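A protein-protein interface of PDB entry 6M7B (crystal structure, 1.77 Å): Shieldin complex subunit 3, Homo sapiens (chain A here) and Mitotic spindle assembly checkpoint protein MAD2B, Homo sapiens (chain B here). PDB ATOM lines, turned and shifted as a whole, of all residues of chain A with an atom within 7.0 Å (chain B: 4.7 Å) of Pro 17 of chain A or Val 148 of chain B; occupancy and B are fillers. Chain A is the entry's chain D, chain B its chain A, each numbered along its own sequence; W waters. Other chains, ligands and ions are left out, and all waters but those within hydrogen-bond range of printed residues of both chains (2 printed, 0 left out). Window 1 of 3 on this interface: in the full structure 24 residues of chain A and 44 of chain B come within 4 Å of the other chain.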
ATOM      1  N   PRO A  14      18.904   8.348  10.114  1.00  0.00           N
ATOM      2  CA  PRO A  14      17.785   8.860   9.323  1.00  0.00           C
ATOM      3  C   PRO A  14      16.590   7.913   9.344  1.00  0.00           C
ATOM      4  O   PRO A  14      16.658   6.779   9.822  1.00  0.00           O
ATOM      5  CB  PRO A  14      18.382   8.938   7.913  1.00  0.00           C
ATOM      6  CG  PRO A  14      19.296   7.783   7.864  1.00  0.00           C
ATOM      7  CD  PRO A  14      19.886   7.639   9.266  1.00  0.00           C
ATOM      8  N   LEU A  15      15.480   8.406   8.816  1.00  0.00           N
ATOM      9  CA  LEU A  15      14.314   7.557   8.634  1.00  0.00           C
ATOM     10  C   LEU A  15      14.335   6.944   7.244  1.00  0.00           C
ATOM     11  O   LEU A  15      14.893   7.517   6.304  1.00  0.00           O
ATOM     12  CB  LEU A  15      13.022   8.348   8.811  1.00  0.00           C
ATOM     13  CG  LEU A  15      12.884   9.014  10.179  1.00  0.00           C
ATOM     14  CD1 LEU A  15      11.783  10.067  10.168  1.00  0.00           C
ATOM     15  CD2 LEU A  15      12.638   7.920  11.205  1.00  0.00           C
ATOM     16  N   ARG A  16      13.666   5.801   7.107  1.00  0.00           N
ATOM     17  CA  ARG A  16      13.510   5.174   5.803  1.00  0.00           C
ATOM     18  C   ARG A  16      12.169   4.459   5.767  1.00  0.00           C
ATOM     19  O   ARG A  16      11.609   4.126   6.818  1.00  0.00           O
ATOM     20  CB  ARG A  16      14.654   4.195   5.506  1.00  0.00           C
ATOM     21  CG  ARG A  16      14.589   2.882   6.298  1.00  0.00           C
ATOM     22  CD  ARG A  16      15.613   1.905   5.718  1.00  0.00           C
ATOM     23  NE  ARG A  16      15.732   0.680   6.500  1.00  0.00           N
ATOM     24  CZ  ARG A  16      14.938  -0.374   6.352  1.00  0.00           C
ATOM     25  NH1 ARG A  16      15.118  -1.459   7.099  1.00  0.00           N
ATOM     26  NH2 ARG A  16      13.958  -0.341   5.455  1.00  0.00           N
ATOM     27  N   PRO A  17      11.629   4.205   4.575  1.00  0.00           N
ATOM     28  CA  PRO A  17      10.411   3.388   4.481  1.00  0.00           C
ATOM     29  C   PRO A  17      10.657   1.975   5.008  1.00  0.00           C
ATOM     30  O   PRO A  17      11.708   1.379   4.774  1.00  0.00           O
ATOM     31  CB  PRO A  17      10.106   3.377   2.977  1.00  0.00           C
ATOM     32  CG  PRO A  17      10.792   4.642   2.434  1.00  0.00           C
ATOM     33  CD  PRO A  17      12.045   4.744   3.264  1.00  0.00           C
ATOM     34  N   LYS A  18       9.674   1.452   5.745  1.00  0.00           N
ATOM     35  CA  LYS A  18       9.691   0.049   6.171  1.00  0.00           C
ATOM     36  C   LYS A  18       9.513  -0.898   4.991  1.00  0.00           C
ATOM     37  O   LYS A  18      10.136  -1.968   4.936  1.00  0.00           O
ATOM     38  CB  LYS A  18       8.565  -0.183   7.189  1.00  0.00           C
ATOM     39  CG  LYS A  18       8.592  -1.522   7.924  1.00  0.00           C
ATOM     40  CD  LYS A  18       9.975  -2.047   8.118  1.00  0.00           C
ATOM     41  CE  LYS A  18      10.050  -2.932   9.342  1.00  0.00           C
ATOM     42  NZ  LYS A  18      11.389  -3.577   9.407  1.00  0.00           N
ATOM     43  N   ARG A  19       8.614  -0.553   4.082  1.00  0.00           N
ATOM     44  CA  ARG A  19       8.382  -1.377   2.909  1.00  0.00           C
ATOM     45  C   ARG A  19       9.594  -1.328   1.990  1.00  0.00           C
ATOM     46  O   ARG A  19      10.359  -0.358   1.982  1.00  0.00           O
ATOM     47  CB  ARG A  19       7.138  -0.902   2.166  1.00  0.00           C
ATOM     48  CG  ARG A  19       5.871  -1.131   2.971  1.00  0.00           C
ATOM     49  CD  ARG A  19       4.694  -0.411   2.361  1.00  0.00           C
ATOM     50  NE  ARG A  19       4.312  -1.018   1.098  1.00  0.00           N
ATOM     51  CZ  ARG A  19       3.071  -1.380   0.799  1.00  0.00           C
ATOM     52  NH1 ARG A  19       2.091  -1.178   1.669  1.00  0.00           N
ATOM     53  NH2 ARG A  19       2.811  -1.940  -0.372  1.00  0.00           N
ATOM     54  N   SER A  20       9.765  -2.373   1.241  1.00  0.00           N
ATOM     55  CA  SER A  20      10.821  -2.476   0.251  1.00  0.00           C
ATOM     56  C   SER A  20      10.261  -2.224  -1.138  1.00  0.00           C
ATOM     57  O   SER A  20       9.098  -2.535  -1.411  1.00  0.00           O
ATOM     58  CB  SER A  20      11.460  -3.869   0.282  1.00  0.00           C
ATOM     59  OG  SER A  20      12.277  -4.018   1.419  1.00  0.00           O
ATOM     60  N   TYR B  63       5.597   2.882  -4.962  1.00  0.00           N
ATOM     61  CA  TYR B  63       6.563   2.988  -3.870  1.00  0.00           C
ATOM     62  C   TYR B  63       7.265   4.344  -3.878  1.00  0.00           C
ATOM     63  O   TYR B  63       7.374   5.019  -2.842  1.00  0.00           O
ATOM     64  CB  TYR B  63       7.578   1.851  -3.992  1.00  0.00           C
ATOM     65  CG  TYR B  63       8.682   1.934  -2.967  1.00  0.00           C
ATOM     66  CD1 TYR B  63       9.849   2.662  -3.225  1.00  0.00           C
ATOM     67  CD2 TYR B  63       8.561   1.288  -1.741  1.00  0.00           C
ATOM     68  CE1 TYR B  63      10.860   2.739  -2.282  1.00  0.00           C
ATOM     69  CE2 TYR B  63       9.567   1.368  -0.797  1.00  0.00           C
ATOM     70  CZ  TYR B  63      10.702   2.091  -1.068  1.00  0.00           C
ATOM     71  OH  TYR B  63      11.701   2.151  -0.123  1.00  0.00           O
ATOM     72  N   THR B  67       6.763   7.287  -1.083  1.00  0.00           N
ATOM     73  CA  THR B  67       7.928   7.743  -0.333  1.00  0.00           C
ATOM     74  C   THR B  67       8.015   9.265  -0.342  1.00  0.00           C
ATOM     75  O   THR B  67       8.139   9.902   0.712  1.00  0.00           O
ATOM     76  CB  THR B  67       9.197   7.105  -0.920  1.00  0.00           C
ATOM     77  OG1 THR B  67       9.112   5.674  -0.806  1.00  0.00           O
ATOM     78  CG2 THR B  67      10.458   7.594  -0.194  1.00  0.00           C
ATOM     79  N   VAL B  83      18.056  14.157   1.521  1.00  0.00           N
ATOM     80  CA  VAL B  83      17.352  12.990   1.003  1.00  0.00           C
ATOM     81  C   VAL B  83      18.372  12.180   0.219  1.00  0.00           C
ATOM     82  O   VAL B  83      19.093  12.736  -0.618  1.00  0.00           O
ATOM     83  CB  VAL B  83      16.157  13.377   0.107  1.00  0.00           C
ATOM     84  CG1 VAL B  83      15.504  12.119  -0.446  1.00  0.00           C
ATOM     85  CG2 VAL B  83      15.098  14.212   0.904  1.00  0.00           C
ATOM     86  N   VAL B  84      18.472  10.883   0.509  1.00  0.00           N
ATOM     87  CA  VAL B  84      19.550  10.061  -0.043  1.00  0.00           C
ATOM     88  C   VAL B  84      18.927   8.859  -0.732  1.00  0.00           C
ATOM     89  O   VAL B  84      18.140   8.140  -0.114  1.00  0.00           O
ATOM     90  CB  VAL B  84      20.524   9.572   1.049  1.00  0.00           C
ATOM     91  CG1 VAL B  84      21.680   8.715   0.448  1.00  0.00           C
ATOM     92  CG2 VAL B  84      21.049  10.738   1.923  1.00  0.00           C
ATOM     93  N   PHE B 146      16.994  -0.761  -3.598  1.00  0.00           N
ATOM     94  CA  PHE B 146      17.363   0.550  -3.077  1.00  0.00           C
ATOM     95  C   PHE B 146      16.478   0.905  -1.900  1.00  0.00           C
ATOM     96  O   PHE B 146      15.490   0.228  -1.607  1.00  0.00           O
ATOM     97  CB  PHE B 146      17.260   1.631  -4.166  1.00  0.00           C
ATOM     98  CG  PHE B 146      15.843   2.005  -4.541  1.00  0.00           C
ATOM     99  CD1 PHE B 146      15.085   1.188  -5.364  1.00  0.00           C
ATOM    100  CD2 PHE B 146      15.294   3.213  -4.105  1.00  0.00           C
ATOM    101  CE1 PHE B 146      13.788   1.535  -5.735  1.00  0.00           C
ATOM    102  CE2 PHE B 146      14.001   3.587  -4.474  1.00  0.00           C
ATOM    103  CZ  PHE B 146      13.241   2.743  -5.289  1.00  0.00           C
ATOM    104  N   THR B 147      16.864   1.976  -1.207  1.00  0.00           N
ATOM    105  CA  THR B 147      15.983   2.612  -0.236  1.00  0.00           C
ATOM    106  C   THR B 147      16.206   4.113  -0.333  1.00  0.00           C
ATOM    107  O   THR B 147      17.076   4.582  -1.071  1.00  0.00           O
ATOM    108  CB  THR B 147      16.198   2.091   1.201  1.00  0.00           C
ATOM    109  OG1 THR B 147      15.132   2.557   2.046  1.00  0.00           O
ATOM    110  CG2 THR B 147      17.526   2.542   1.792  1.00  0.00           C
ATOM    111  N   VAL B 148      15.370   4.868   0.375  1.00  0.00           N
ATOM    112  CA  VAL B 148      15.488   6.320   0.460  1.00  0.00           C
ATOM    113  C   VAL B 148      15.655   6.680   1.931  1.00  0.00           C
ATOM    114  O   VAL B 148      14.855   6.250   2.768  1.00  0.00           O
ATOM    115  CB  VAL B 148      14.260   7.031  -0.135  1.00  0.00           C
ATOM    116  CG1 VAL B 148      14.374   8.545   0.067  1.00  0.00           C
ATOM    117  CG2 VAL B 148      14.093   6.668  -1.613  1.00  0.00           C
ATOM    118  N   LEU B 149      16.677   7.471   2.241  1.00  0.00           N
ATOM    119  CA  LEU B 149      16.931   7.941   3.597  1.00  0.00           C
ATOM    120  C   LEU B 149      16.579   9.414   3.708  1.00  0.00           C
ATOM    121  O   LEU B 149      16.907  10.208   2.818  1.00  0.00           O
ATOM    122  CB  LEU B 149      18.393   7.761   3.989  1.00  0.00           C
ATOM    123  CG  LEU B 149      19.001   6.386   3.743  1.00  0.00           C
ATOM    124  CD1 LEU B 149      20.461   6.453   4.139  1.00  0.00           C
ATOM    125  CD2 LEU B 149      18.262   5.344   4.572  1.00  0.00           C
ATOM    126  N   VAL B 150      15.916   9.774   4.811  1.00  0.00           N
ATOM    127  CA  VAL B 150      15.530  11.150   5.095  1.00  0.00           C
ATOM    128  C   VAL B 150      16.226  11.562   6.385  1.00  0.00           C
ATOM    129  O   VAL B 150      15.871  11.084   7.473  1.00  0.00           O
ATOM    130  CB  VAL B 150      14.006  11.306   5.207  1.00  0.00           C
ATOM    131  CG1 VAL B 150      13.638  12.756   5.550  1.00  0.00           C
ATOM    132  CG2 VAL B 150      13.330  10.885   3.890  1.00  0.00           C
ATOM    133  N   PHE B 169       1.941   2.654   4.909  1.00  0.00           N
ATOM    134  CA  PHE B 169       3.293   2.927   4.404  1.00  0.00           C
ATOM    135  C   PHE B 169       4.147   3.437   5.563  1.00  0.00           C
ATOM    136  O   PHE B 169       4.526   4.616   5.608  1.00  0.00           O
ATOM    137  CB  PHE B 169       3.274   3.929   3.243  1.00  0.00           C
ATOM    138  CG  PHE B 169       4.521   3.902   2.392  1.00  0.00           C
ATOM    139  CD1 PHE B 169       4.646   2.993   1.350  1.00  0.00           C
ATOM    140  CD2 PHE B 169       5.579   4.782   2.644  1.00  0.00           C
ATOM    141  CE1 PHE B 169       5.787   2.943   0.575  1.00  0.00           C
ATOM    142  CE2 PHE B 169       6.742   4.743   1.860  1.00  0.00           C
ATOM    143  CZ  PHE B 169       6.847   3.830   0.828  1.00  0.00           C
ATOM    144  N   PRO B 170       4.486   2.569   6.509  1.00  0.00           N
ATOM    145  CA  PRO B 170       5.177   3.025   7.721  1.00  0.00           C
ATOM    146  C   PRO B 170       6.636   3.341   7.451  1.00  0.00           C
ATOM    147  O   PRO B 170       7.246   2.846   6.507  1.00  0.00           O
ATOM    148  CB  PRO B 170       5.053   1.835   8.677  1.00  0.00           C
ATOM    149  CG  PRO B 170       4.945   0.640   7.767  1.00  0.00           C
ATOM    150  CD  PRO B 170       4.257   1.109   6.512  1.00  0.00           C
ATOM    151  N   TRP B 171       7.190   4.180   8.319  1.00  0.00           N
ATOM    152  CA  TRP B 171       8.598   4.533   8.288  1.00  0.00           C
ATOM    153  C   TRP B 171       9.252   4.051   9.573  1.00  0.00           C
ATOM    154  O   TRP B 171       8.582   3.845  10.589  1.00  0.00           O
ATOM    155  CB  TRP B 171       8.795   6.050   8.126  1.00  0.00           C
ATOM    156  CG  TRP B 171       8.467   6.579   6.738  1.00  0.00           C
ATOM    157  CD1 TRP B 171       7.224   6.620   6.144  1.00  0.00           C
ATOM    158  CD2 TRP B 171       9.384   7.146   5.785  1.00  0.00           C
ATOM    159  NE1 TRP B 171       7.319   7.180   4.886  1.00  0.00           N
ATOM    160  CE2 TRP B 171       8.630   7.514   4.643  1.00  0.00           C
ATOM    161  CE3 TRP B 171      10.762   7.403   5.795  1.00  0.00           C
ATOM    162  CZ2 TRP B 171       9.213   8.114   3.524  1.00  0.00           C
ATOM    163  CZ3 TRP B 171      11.345   7.993   4.677  1.00  0.00           C
ATOM    164  CH2 TRP B 171      10.571   8.333   3.548  1.00  0.00           C
ATOM    165  N   ILE B 172      10.572   3.843   9.513  1.00  0.00           N
ATOM    166  CA  ILE B 172      11.348   3.376  10.659  1.00  0.00           C
ATOM    167  C   ILE B 172      12.679   4.110  10.652  1.00  0.00           C
ATOM    168  O   ILE B 172      13.133   4.613   9.615  1.00  0.00           O
ATOM    169  CB  ILE B 172      11.619   1.854  10.609  1.00  0.00           C
ATOM    170  CG1 ILE B 172      12.242   1.497   9.260  1.00  0.00           C
ATOM    171  CG2 ILE B 172      10.333   1.063  10.848  1.00  0.00           C
ATOM    172  CD1 ILE B 172      12.856   0.111   9.204  1.00  0.00           C
HETATM  173  O   HOH W   1      12.920   1.059   2.009  1.00  0.00           O
HETATM  174  O   HOH W   2       6.877   1.781   4.028  1.00  0.00           O
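The backbone carbonyl oxygen of Leu 15 of chain A lies within hydrogen-bond range of the backbone NH of Val 150 of chain B (2.9 Å).
O of Pro 170 of chain B lies within hydrogen-bond range of N of Lys 18 of chain A, at 2.9 Å.
The backbone NH (N) of Arg 16 of chain A is in hydrogen-bond range of the backbone carbonyl oxygen (O) of Ile 172 of chain B (2.8 Å).
Among the printed residues, pairs that only touch across the chains: Pro 14 of chain A with Leu 149 of chain B (3.98 Å), Pro 14 of chain A with Val 150 of chain B (3.3 Å), Leu 15 of chain A with Val 148 of chain B (3.8 Å), Leu 15 of chain A with Leu 149 of chain B (3.4 Å), Leu 15 of chain A with Trp 171 of chain B (3.9 Å), Leu 15 of chain A with Ile 172 of chain B (3.3 Å), Arg 16 of chain A with Thr 147 of chain B (3.8 Å), Arg 16 of chain A with Val 148 of chain B (3.4 Å), Arg 16 of chain A with Leu 149 of chain B (3.9 Å), Arg 16 of chain A with Trp 171 of chain B (3.3 Å), Pro 17 of chain A with Tyr 63 of chain B (3.7 Å), Pro 17 of chain A with Thr 67 of chain B (3.8 Å), Pro 17 of chain A with Thr 147 of chain B (3.97 Å), Pro 17 of chain A with Val 148 of chain B (3.2 Å), Pro 17 of chain A with Phe 169 of chain B (3.8 Å), Pro 17 of chain A with Pro 170 of chain B (3.8 Å), Pro 17 of chain A with Trp 171 of chain B (3.5 Å), Lys 18 of chain A with Ile 172 of chain B (3.8 Å), Arg 19 of chain A with Tyr 63 of chain B (3.4 Å), Arg 19 of chain A with Phe 169 of chain B (3.6 Å) and Ser 20 of chain A with Tyr 63 of chain B (3.7 Å).
Of the printed residues of chain B, Pro 17 of chain A touches Tyr 63 (3.7 Å), Thr 67 (3.8 Å), Thr 147 (3.97 Å), Val 148 (3.2 Å), Phe 169 (3.8 Å), Pro 170 (3.8 Å) and Trp 171 (3.5 Å).
Val 148 of chain B touches just these residues of chain A: Leu 15 (3.8 Å), Arg 16 (3.4 Å) and Pro 17 (3.2 Å).
Of the printed residues of chain A, Val 150 of chain B touches Pro 14 and Leu 15.
Of the printed residues of chain B, Arg 19 of chain A touches Tyr 63 (3.4 Å) and Phe 169 (3.6 Å).
Printed residues of chain B within 4 Å of Leu 15 of chain A: Val 148 (3.8 Å), Leu 149 (3.4 Å), Val 150 (2.9 Å), Trp 171 (3.9 Å) and Ile 172 (3.3 Å).
Val 84 of chain B touches none of the printed residues of chain A.
Val 83 of chain B touches none of the printed residues of chain A.
The nearest residue of chain B that does not touch Pro 17 of chain A is Ile 172 of chain B (4.5 Å).
The nearest residue of chain A that does not touch Val 148 of chain B is Pro 14 of chain A (6.8 Å).
The nearest printed residue of chain A that does not touch Trp 171 of chain B is Lys 18 of chain A (4.1 Å).
O of Tyr 63 of chain B lies within hydrogen-bond range of OG1 of Thr 67 of chain B.
O of Val 84 of chain B sits at hydrogen-bond distance from N of Leu 149 of chain B (2.9 Å).
Water W1 lies within hydrogen-bond range of OG1 of Thr 147 of chain B, OH of Tyr 63 of chain B, O of Arg 19 of chain A and O of Pro 17 of chain A.
Water W2 lies within hydrogen-bond range of the backbone carbonyl oxygen of Pro 170 of chain B (2.7 Å), the backbone NH of Arg 19 of chain A (2.9 Å) and the backbone NH of Lys 18 of chain A (3.3 Å).
Printed residues of chain B that touch a printed residue of chain A: Tyr 63, Thr 67, Thr 147, Val 148, Leu 149, Val 150, Phe 169, Pro 170, Trp 171 and Ile 172.
Along chain B the printed residues that touch a printed residue of chain A span positions 63 to 172.
Of the 7 printed residues of chain A, 7 touch a printed residue of chain B.
Hydrophobic or aromatic side chains of chain A within 4 Å of the printed part of chain B: Pro 14, Leu 15 and Pro 17.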
